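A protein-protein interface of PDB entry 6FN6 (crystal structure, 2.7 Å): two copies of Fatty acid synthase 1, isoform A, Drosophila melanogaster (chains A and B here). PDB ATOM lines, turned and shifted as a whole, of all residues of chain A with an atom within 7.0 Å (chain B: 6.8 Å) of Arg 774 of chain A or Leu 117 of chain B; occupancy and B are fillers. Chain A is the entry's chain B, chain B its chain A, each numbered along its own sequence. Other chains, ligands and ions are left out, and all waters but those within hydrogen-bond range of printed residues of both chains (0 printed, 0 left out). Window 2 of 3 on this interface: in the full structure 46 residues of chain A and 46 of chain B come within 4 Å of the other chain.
OE1 of Glu 240 of chain B sits at hydrogen-bond distance from N of Leu 115 of chain B (3.0 Å). The side-chain amide oxygen (OE1) of Gln 770 of chain A lies close to the backbone carbonyl oxygen (O) of Ser 767 of chain A (3.3 Å). O of Leu 773 of chain A is in hydrogen-bond range of N of Gly 778 of chain A (2.9 Å).
Among the printed residues, merely in contact across the chains: Gln 770 of chain A with Leu 115 of chain B (3.9 Å), Gln 770 of chain A with Ile 231 of chain B (3.8 Å), Leu 773 of chain A with Asp 230 of chain B (3.5 Å), Leu 773 of chain A with Ile 231 of chain B (3.9 Å), Arg 774 of chain A with Leu 117 of chain B (3.5 Å), Arg 774 of chain A with Asp 230 of chain B (3.9 Å), Lys 777 of chain A with Asp 230 of chain B (3.4 Å) and Gly 778 of chain A with Asp 230 of chain B (3.9 Å).
Of chain B, only Leu 117 and Asp 230 come within 4 Å of Arg 774 of chain A. Leu 117 of chain B touches just one residue of chain A: Arg 774 (3.5 Å). Of the printed residues of chain A, Leu 115 of chain B touches Gln 770 (3.9 Å). Of the printed residues of chain B, Gly 778 of chain A touches Asp 230 (3.9 Å). Val 233 of chain B touches none of the printed residues of chain A.
Of the 13 printed residues of chain A, 5 touch a printed residue of chain B. Along chain B the printed residues that touch a printed residue of chain A span positions 115 to 231. Among the printed residues, 8 pairs touch across the chains.
No position is printed for both chains. Of the 8 pairs that touch across the chains among the printed residues, none has its exchanged pair printed and touching as well.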
ATOM      1  N   ARG A 758       5.985 -13.783  21.818  1.00  0.00           N
ATOM      2  CA  ARG A 758       7.362 -14.247  21.921  1.00  0.00           C
ATOM      3  C   ARG A 758       7.742 -14.501  23.379  1.00  0.00           C
ATOM      4  O   ARG A 758       8.629 -15.305  23.665  1.00  0.00           O
ATOM      5  CB  ARG A 758       8.329 -13.235  21.299  1.00  0.00           C
ATOM      6  CG  ARG A 758       8.174 -13.059  19.795  1.00  0.00           C
ATOM      7  CD  ARG A 758       9.116 -11.990  19.255  1.00  0.00           C
ATOM      8  NE  ARG A 758      10.520 -12.340  19.471  1.00  0.00           N
ATOM      9  CZ  ARG A 758      11.243 -13.102  18.653  1.00  0.00           C
ATOM     10  NH1 ARG A 758      10.703 -13.611  17.553  1.00  0.00           N
ATOM     11  NH2 ARG A 758      12.512 -13.361  18.938  1.00  0.00           N
ATOM     12  N   SER A 767      10.805 -26.265  28.168  1.00  0.00           N
ATOM     13  CA  SER A 767      11.070 -25.477  26.967  1.00  0.00           C
ATOM     14  C   SER A 767      11.231 -23.981  27.238  1.00  0.00           C
ATOM     15  O   SER A 767      11.925 -23.288  26.494  1.00  0.00           O
ATOM     16  CB  SER A 767       9.951 -25.685  25.945  1.00  0.00           C
ATOM     17  OG  SER A 767       8.766 -25.018  26.344  1.00  0.00           O
ATOM     18  N   PHE A 768      10.592 -23.476  28.288  1.00  0.00           N
ATOM     19  CA  PHE A 768      10.612 -22.039  28.552  1.00  0.00           C
ATOM     20  C   PHE A 768      12.035 -21.540  28.810  1.00  0.00           C
ATOM     21  O   PHE A 768      12.320 -20.354  28.651  1.00  0.00           O
ATOM     22  CB  PHE A 768       9.707 -21.685  29.738  1.00  0.00           C
ATOM     23  CG  PHE A 768      10.171 -22.246  31.055  1.00  0.00           C
ATOM     24  CD1 PHE A 768      11.139 -21.590  31.801  1.00  0.00           C
ATOM     25  CD2 PHE A 768       9.630 -23.420  31.554  1.00  0.00           C
ATOM     26  CE1 PHE A 768      11.565 -22.101  33.010  1.00  0.00           C
ATOM     27  CE2 PHE A 768      10.052 -23.934  32.764  1.00  0.00           C
ATOM     28  CZ  PHE A 768      11.020 -23.273  33.494  1.00  0.00           C
ATOM     29  N   GLU A 769      12.922 -22.442  29.218  1.00  0.00           N
ATOM     30  CA  GLU A 769      14.318 -22.082  29.440  1.00  0.00           C
ATOM     31  C   GLU A 769      14.942 -21.586  28.140  1.00  0.00           C
ATOM     32  O   GLU A 769      15.574 -20.532  28.102  1.00  0.00           O
ATOM     33  CB  GLU A 769      15.104 -23.277  29.984  1.00  0.00           C
ATOM     34  CG  GLU A 769      16.555 -22.964  30.303  1.00  0.00           C
ATOM     35  CD  GLU A 769      17.332 -24.188  30.741  1.00  0.00           C
ATOM     36  OE1 GLU A 769      16.698 -25.169  31.184  1.00  0.00           O
ATOM     37  OE2 GLU A 769      18.578 -24.173  30.636  1.00  0.00           O
ATOM     38  N   GLN A 770      14.760 -22.362  27.077  1.00  0.00           N
ATOM     39  CA  GLN A 770      15.301 -22.016  25.768  1.00  0.00           C
ATOM     40  C   GLN A 770      14.696 -20.716  25.252  1.00  0.00           C
ATOM     41  O   GLN A 770      15.400 -19.866  24.715  1.00  0.00           O
ATOM     42  CB  GLN A 770      15.047 -23.149  24.772  1.00  0.00           C
ATOM     43  CG  GLN A 770      15.927 -24.373  24.986  1.00  0.00           C
ATOM     44  CD  GLN A 770      15.593 -25.113  26.265  1.00  0.00           C
ATOM     45  OE1 GLN A 770      14.429 -25.379  26.553  1.00  0.00           O
ATOM     46  NE2 GLN A 770      16.618 -25.446  27.042  1.00  0.00           N
ATOM     47  N   LEU A 771      13.389 -20.568  25.423  1.00  0.00           N
ATOM     48  CA  LEU A 771      12.681 -19.380  24.955  1.00  0.00           C
ATOM     49  C   LEU A 771      13.239 -18.126  25.620  1.00  0.00           C
ATOM     50  O   LEU A 771      13.498 -17.121  24.959  1.00  0.00           O
ATOM     51  CB  LEU A 771      11.181 -19.512  25.234  1.00  0.00           C
ATOM     52  CG  LEU A 771      10.265 -18.365  24.798  1.00  0.00           C
ATOM     53  CD1 LEU A 771       8.884 -18.911  24.462  1.00  0.00           C
ATOM     54  CD2 LEU A 771      10.149 -17.278  25.864  1.00  0.00           C
ATOM     55  N   VAL A 772      13.405 -18.185  26.937  1.00  0.00           N
ATOM     56  CA  VAL A 772      13.859 -17.036  27.707  1.00  0.00           C
ATOM     57  C   VAL A 772      15.306 -16.683  27.371  1.00  0.00           C
ATOM     58  O   VAL A 772      15.621 -15.519  27.129  1.00  0.00           O
ATOM     59  CB  VAL A 772      13.690 -17.299  29.218  1.00  0.00           C
ATOM     60  CG1 VAL A 772      14.389 -16.221  30.046  1.00  0.00           C
ATOM     61  CG2 VAL A 772      12.213 -17.377  29.579  1.00  0.00           C
ATOM     62  N   LEU A 773      16.183 -17.681  27.355  1.00  0.00           N
ATOM     63  CA  LEU A 773      17.592 -17.440  27.056  1.00  0.00           C
ATOM     64  C   LEU A 773      17.756 -16.889  25.642  1.00  0.00           C
ATOM     65  O   LEU A 773      18.625 -16.054  25.391  1.00  0.00           O
ATOM     66  CB  LEU A 773      18.417 -18.720  27.219  1.00  0.00           C
ATOM     67  CG  LEU A 773      18.575 -19.287  28.633  1.00  0.00           C
ATOM     68  CD1 LEU A 773      19.383 -20.578  28.598  1.00  0.00           C
ATOM     69  CD2 LEU A 773      19.220 -18.281  29.572  1.00  0.00           C
ATOM     70  N   ARG A 774      16.926 -17.359  24.718  1.00  0.00           N
ATOM     71  CA  ARG A 774      16.973 -16.871  23.343  1.00  0.00           C
ATOM     72  C   ARG A 774      16.561 -15.403  23.281  1.00  0.00           C
ATOM     73  O   ARG A 774      17.179 -14.608  22.576  1.00  0.00           O
ATOM     74  CB  ARG A 774      16.078 -17.718  22.431  1.00  0.00           C
ATOM     75  CG  ARG A 774      16.863 -18.565  21.440  1.00  0.00           C
ATOM     76  CD  ARG A 774      15.977 -19.181  20.369  1.00  0.00           C
ATOM     77  NE  ARG A 774      15.144 -20.265  20.887  1.00  0.00           N
ATOM     78  CZ  ARG A 774      15.491 -21.548  20.879  1.00  0.00           C
ATOM     79  NH1 ARG A 774      16.665 -21.930  20.385  1.00  0.00           N
ATOM     80  NH2 ARG A 774      14.663 -22.460  21.371  1.00  0.00           N
ATOM     81  N   GLU A 775      15.510 -15.053  24.014  1.00  0.00           N
ATOM     82  CA  GLU A 775      14.972 -13.697  23.986  1.00  0.00           C
ATOM     83  C   GLU A 775      15.814 -12.725  24.808  1.00  0.00           C
ATOM     84  O   GLU A 775      15.760 -11.515  24.590  1.00  0.00           O
ATOM     85  CB  GLU A 775      13.529 -13.690  24.496  1.00  0.00           C
ATOM     86  CG  GLU A 775      12.544 -14.385  23.569  1.00  0.00           C
ATOM     87  CD  GLU A 775      12.448 -13.710  22.215  1.00  0.00           C
ATOM     88  OE1 GLU A 775      12.546 -14.414  21.189  1.00  0.00           O
ATOM     89  OE2 GLU A 775      12.274 -12.474  22.179  1.00  0.00           O
ATOM     90  N   THR A 776      16.578 -13.252  25.762  1.00  0.00           N
ATOM     91  CA  THR A 776      17.464 -12.421  26.571  1.00  0.00           C
ATOM     92  C   THR A 776      18.916 -12.535  26.108  1.00  0.00           C
ATOM     93  O   THR A 776      19.818 -11.960  26.719  1.00  0.00           O
ATOM     94  CB  THR A 776      17.388 -12.802  28.058  1.00  0.00           C
ATOM     95  OG1 THR A 776      17.727 -14.186  28.219  1.00  0.00           O
ATOM     96  CG2 THR A 776      15.985 -12.554  28.600  1.00  0.00           C
ATOM     97  N   LYS A 777      19.133 -13.275  25.025  1.00  0.00           N
ATOM     98  CA  LYS A 777      20.465 -13.449  24.457  1.00  0.00           C
ATOM     99  C   LYS A 777      21.483 -13.922  25.494  1.00  0.00           C
ATOM    100  O   LYS A 777      22.625 -13.464  25.512  1.00  0.00           O
ATOM    101  CB  LYS A 777      20.938 -12.143  23.818  1.00  0.00           C
ATOM    102  CG  LYS A 777      20.282 -11.857  22.479  1.00  0.00           C
ATOM    103  CD  LYS A 777      20.862 -10.618  21.822  1.00  0.00           C
ATOM    104  CE  LYS A 777      20.555 -10.588  20.335  1.00  0.00           C
ATOM    105  NZ  LYS A 777      21.286  -9.497  19.633  1.00  0.00           N
ATOM    106  N   GLY A 778      21.063 -14.843  26.356  1.00  0.00           N
ATOM    107  CA  GLY A 778      21.958 -15.437  27.333  1.00  0.00           C
ATOM    108  C   GLY A 778      22.083 -14.646  28.619  1.00  0.00           C
ATOM    109  O   GLY A 778      22.669 -15.120  29.592  1.00  0.00           O
ATOM    110  N   GLU B 114      14.698 -34.327  22.747  1.00  0.00           N
ATOM    111  CA  GLU B 114      15.616 -33.466  22.000  1.00  0.00           C
ATOM    112  C   GLU B 114      15.020 -32.083  21.756  1.00  0.00           C
ATOM    113  O   GLU B 114      13.810 -31.892  21.875  1.00  0.00           O
ATOM    114  CB  GLU B 114      15.978 -34.112  20.662  1.00  0.00           C
ATOM    115  CG  GLU B 114      16.452 -35.548  20.784  1.00  0.00           C
ATOM    116  CD  GLU B 114      17.304 -35.987  19.611  1.00  0.00           C
ATOM    117  OE1 GLU B 114      16.759 -36.620  18.682  1.00  0.00           O
ATOM    118  OE2 GLU B 114      18.521 -35.704  19.622  1.00  0.00           O
ATOM    119  N   LEU B 115      15.876 -31.123  21.411  1.00  0.00           N
ATOM    120  CA  LEU B 115      15.427 -29.765  21.117  1.00  0.00           C
ATOM    121  C   LEU B 115      15.274 -29.569  19.608  1.00  0.00           C
ATOM    122  O   LEU B 115      16.122 -30.025  18.835  1.00  0.00           O
ATOM    123  CB  LEU B 115      16.411 -28.734  21.679  1.00  0.00           C
ATOM    124  CG  LEU B 115      16.521 -28.596  23.200  1.00  0.00           C
ATOM    125  CD1 LEU B 115      17.673 -27.672  23.560  1.00  0.00           C
ATOM    126  CD2 LEU B 115      15.224 -28.077  23.796  1.00  0.00           C
ATOM    127  N   PRO B 116      14.201 -28.877  19.180  1.00  0.00           N
ATOM    128  CA  PRO B 116      13.991 -28.600  17.754  1.00  0.00           C
ATOM    129  C   PRO B 116      14.861 -27.450  17.257  1.00  0.00           C
ATOM    130  O   PRO B 116      14.387 -26.317  17.167  1.00  0.00           O
ATOM    131  CB  PRO B 116      12.508 -28.242  17.686  1.00  0.00           C
ATOM    132  CG  PRO B 116      12.220 -27.633  19.006  1.00  0.00           C
ATOM    133  CD  PRO B 116      13.087 -28.363  19.999  1.00  0.00           C
ATOM    134  N   LEU B 117      16.117 -27.742  16.936  1.00  0.00           N
ATOM    135  CA  LEU B 117      17.071 -26.705  16.565  1.00  0.00           C
ATOM    136  C   LEU B 117      17.461 -26.819  15.096  1.00  0.00           C
ATOM    137  O   LEU B 117      17.774 -27.905  14.607  1.00  0.00           O
ATOM    138  CB  LEU B 117      18.317 -26.795  17.447  1.00  0.00           C
ATOM    139  CG  LEU B 117      18.102 -26.420  18.916  1.00  0.00           C
ATOM    140  CD1 LEU B 117      19.276 -26.887  19.764  1.00  0.00           C
ATOM    141  CD2 LEU B 117      17.877 -24.925  19.079  1.00  0.00           C
ATOM    142  N   GLU B 118      17.441 -25.685  14.401  1.00  0.00           N
ATOM    143  CA  GLU B 118      17.827 -25.632  12.998  1.00  0.00           C
ATOM    144  C   GLU B 118      19.261 -25.134  12.845  1.00  0.00           C
ATOM    145  O   GLU B 118      19.766 -24.396  13.692  1.00  0.00           O
ATOM    146  CB  GLU B 118      16.870 -24.728  12.218  1.00  0.00           C
ATOM    147  CG  GLU B 118      15.514 -25.358  11.934  1.00  0.00           C
ATOM    148  CD  GLU B 118      15.592 -26.468  10.904  1.00  0.00           C
ATOM    149  OE1 GLU B 118      16.700 -26.724  10.388  1.00  0.00           O
ATOM    150  OE2 GLU B 118      14.544 -27.083  10.610  1.00  0.00           O
ATOM    151  N   GLU B 119      19.910 -25.552  11.763  1.00  0.00           N
ATOM    152  CA  GLU B 119      21.298 -25.187  11.498  1.00  0.00           C
ATOM    153  C   GLU B 119      21.506 -23.675  11.469  1.00  0.00           C
ATOM    154  O   GLU B 119      20.624 -22.921  11.060  1.00  0.00           O
ATOM    155  CB  GLU B 119      21.758 -25.791  10.170  1.00  0.00           C
ATOM    156  CG  GLU B 119      21.921 -27.303  10.197  1.00  0.00           C
ATOM    157  CD  GLU B 119      22.575 -27.843   8.938  1.00  0.00           C
ATOM    158  OE1 GLU B 119      23.651 -27.333   8.560  1.00  0.00           O
ATOM    159  OE2 GLU B 119      22.013 -28.775   8.326  1.00  0.00           O
ATOM    160  N   GLN B 226      26.917 -27.933  15.830  1.00  0.00           N
ATOM    161  CA  GLN B 226      26.384 -26.600  16.096  1.00  0.00           C
ATOM    162  C   GLN B 226      26.657 -26.167  17.530  1.00  0.00           C
ATOM    163  O   GLN B 226      26.626 -26.980  18.451  1.00  0.00           O
ATOM    164  CB  GLN B 226      24.880 -26.560  15.822  1.00  0.00           C
ATOM    165  CG  GLN B 226      24.481 -27.038  14.436  1.00  0.00           C
ATOM    166  CD  GLN B 226      24.910 -26.078  13.345  1.00  0.00           C
ATOM    167  OE1 GLN B 226      25.070 -24.881  13.584  1.00  0.00           O
ATOM    168  NE2 GLN B 226      25.096 -26.598  12.138  1.00  0.00           N
ATOM    169  N   TYR B 228      25.182 -23.246  20.032  1.00  0.00           N
ATOM    170  CA  TYR B 228      24.250 -22.164  20.343  1.00  0.00           C
ATOM    171  C   TYR B 228      24.610 -21.536  21.687  1.00  0.00           C
ATOM    172  O   TYR B 228      24.337 -22.107  22.740  1.00  0.00           O
ATOM    173  CB  TYR B 228      22.814 -22.684  20.367  1.00  0.00           C
ATOM    174  CG  TYR B 228      22.435 -23.486  19.142  1.00  0.00           C
ATOM    175  CD1 TYR B 228      22.671 -24.854  19.084  1.00  0.00           C
ATOM    176  CD2 TYR B 228      21.839 -22.878  18.046  1.00  0.00           C
ATOM    177  CE1 TYR B 228      22.328 -25.592  17.968  1.00  0.00           C
ATOM    178  CE2 TYR B 228      21.491 -23.610  16.923  1.00  0.00           C
ATOM    179  CZ  TYR B 228      21.738 -24.966  16.891  1.00  0.00           C
ATOM    180  OH  TYR B 228      21.394 -25.699  15.778  1.00  0.00           O
ATOM    181  N   ASP B 230      23.540 -18.831  23.281  1.00  0.00           N
ATOM    182  CA  ASP B 230      22.470 -18.309  24.126  1.00  0.00           C
ATOM    183  C   ASP B 230      21.906 -19.387  25.052  1.00  0.00           C
ATOM    184  O   ASP B 230      21.744 -19.159  26.251  1.00  0.00           O
ATOM    185  CB  ASP B 230      21.342 -17.726  23.272  1.00  0.00           C
ATOM    186  CG  ASP B 230      21.749 -16.454  22.560  1.00  0.00           C
ATOM    187  OD1 ASP B 230      22.963 -16.162  22.518  1.00  0.00           O
ATOM    188  OD2 ASP B 230      20.855 -15.750  22.042  1.00  0.00           O
ATOM    189  N   ILE B 231      21.608 -20.554  24.489  1.00  0.00           N
ATOM    190  CA  ILE B 231      21.000 -21.642  25.250  1.00  0.00           C
ATOM    191  C   ILE B 231      22.053 -22.617  25.775  1.00  0.00           C
ATOM    192  O   ILE B 231      21.741 -23.511  26.561  1.00  0.00           O
ATOM    193  CB  ILE B 231      19.945 -22.383  24.402  1.00  0.00           C
ATOM    194  CG1 ILE B 231      20.585 -22.986  23.147  1.00  0.00           C
ATOM    195  CG2 ILE B 231      18.821 -21.426  24.017  1.00  0.00           C
ATOM    196  CD1 ILE B 231      19.666 -23.911  22.371  1.00  0.00           C
ATOM    197  N   VAL B 233      24.171 -25.026  24.060  1.00  0.00           N
ATOM    198  CA  VAL B 233      23.963 -26.377  23.552  1.00  0.00           C
ATOM    199  C   VAL B 233      24.944 -26.703  22.427  1.00  0.00           C
ATOM    200  O   VAL B 233      25.192 -25.882  21.547  1.00  0.00           O
ATOM    201  CB  VAL B 233      22.506 -26.563  23.070  1.00  0.00           C
ATOM    202  CG1 VAL B 233      22.303 -27.955  22.475  1.00  0.00           C
ATOM    203  CG2 VAL B 233      21.535 -26.331  24.211  1.00  0.00           C
ATOM    204  N   LYS B 235      25.184 -29.440  19.507  1.00  0.00           N
ATOM    205  CA  LYS B 235      24.366 -30.452  18.848  1.00  0.00           C
ATOM    206  C   LYS B 235      24.986 -30.961  17.548  1.00  0.00           C
ATOM    207  O   LYS B 235      25.327 -30.178  16.660  1.00  0.00           O
ATOM    208  CB  LYS B 235      22.970 -29.894  18.571  1.00  0.00           C
ATOM    209  CG  LYS B 235      21.960 -30.956  18.180  1.00  0.00           C
ATOM    210  CD  LYS B 235      20.538 -30.424  18.212  1.00  0.00           C
ATOM    211  CE  LYS B 235      19.542 -31.495  17.787  1.00  0.00           C
ATOM    212  NZ  LYS B 235      19.656 -32.741  18.601  1.00  0.00           N
ATOM    213  N   GLU B 240      23.235 -34.624  21.702  1.00  0.00           N
ATOM    214  CA  GLU B 240      22.867 -33.267  22.089  1.00  0.00           C
ATOM    215  C   GLU B 240      23.365 -32.978  23.505  1.00  0.00           C
ATOM    216  O   GLU B 240      22.969 -33.649  24.458  1.00  0.00           O
ATOM    217  CB  GLU B 240      21.351 -33.083  22.002  1.00  0.00           C
ATOM    218  CG  GLU B 240      20.892 -31.644  22.103  1.00  0.00           C
ATOM    219  CD  GLU B 240      19.381 -31.515  22.125  1.00  0.00           C
ATOM    220  OE1 GLU B 240      18.755 -31.661  21.055  1.00  0.00           O
ATOM    221  OE2 GLU B 240      18.821 -31.263  23.211  1.00  0.00           O
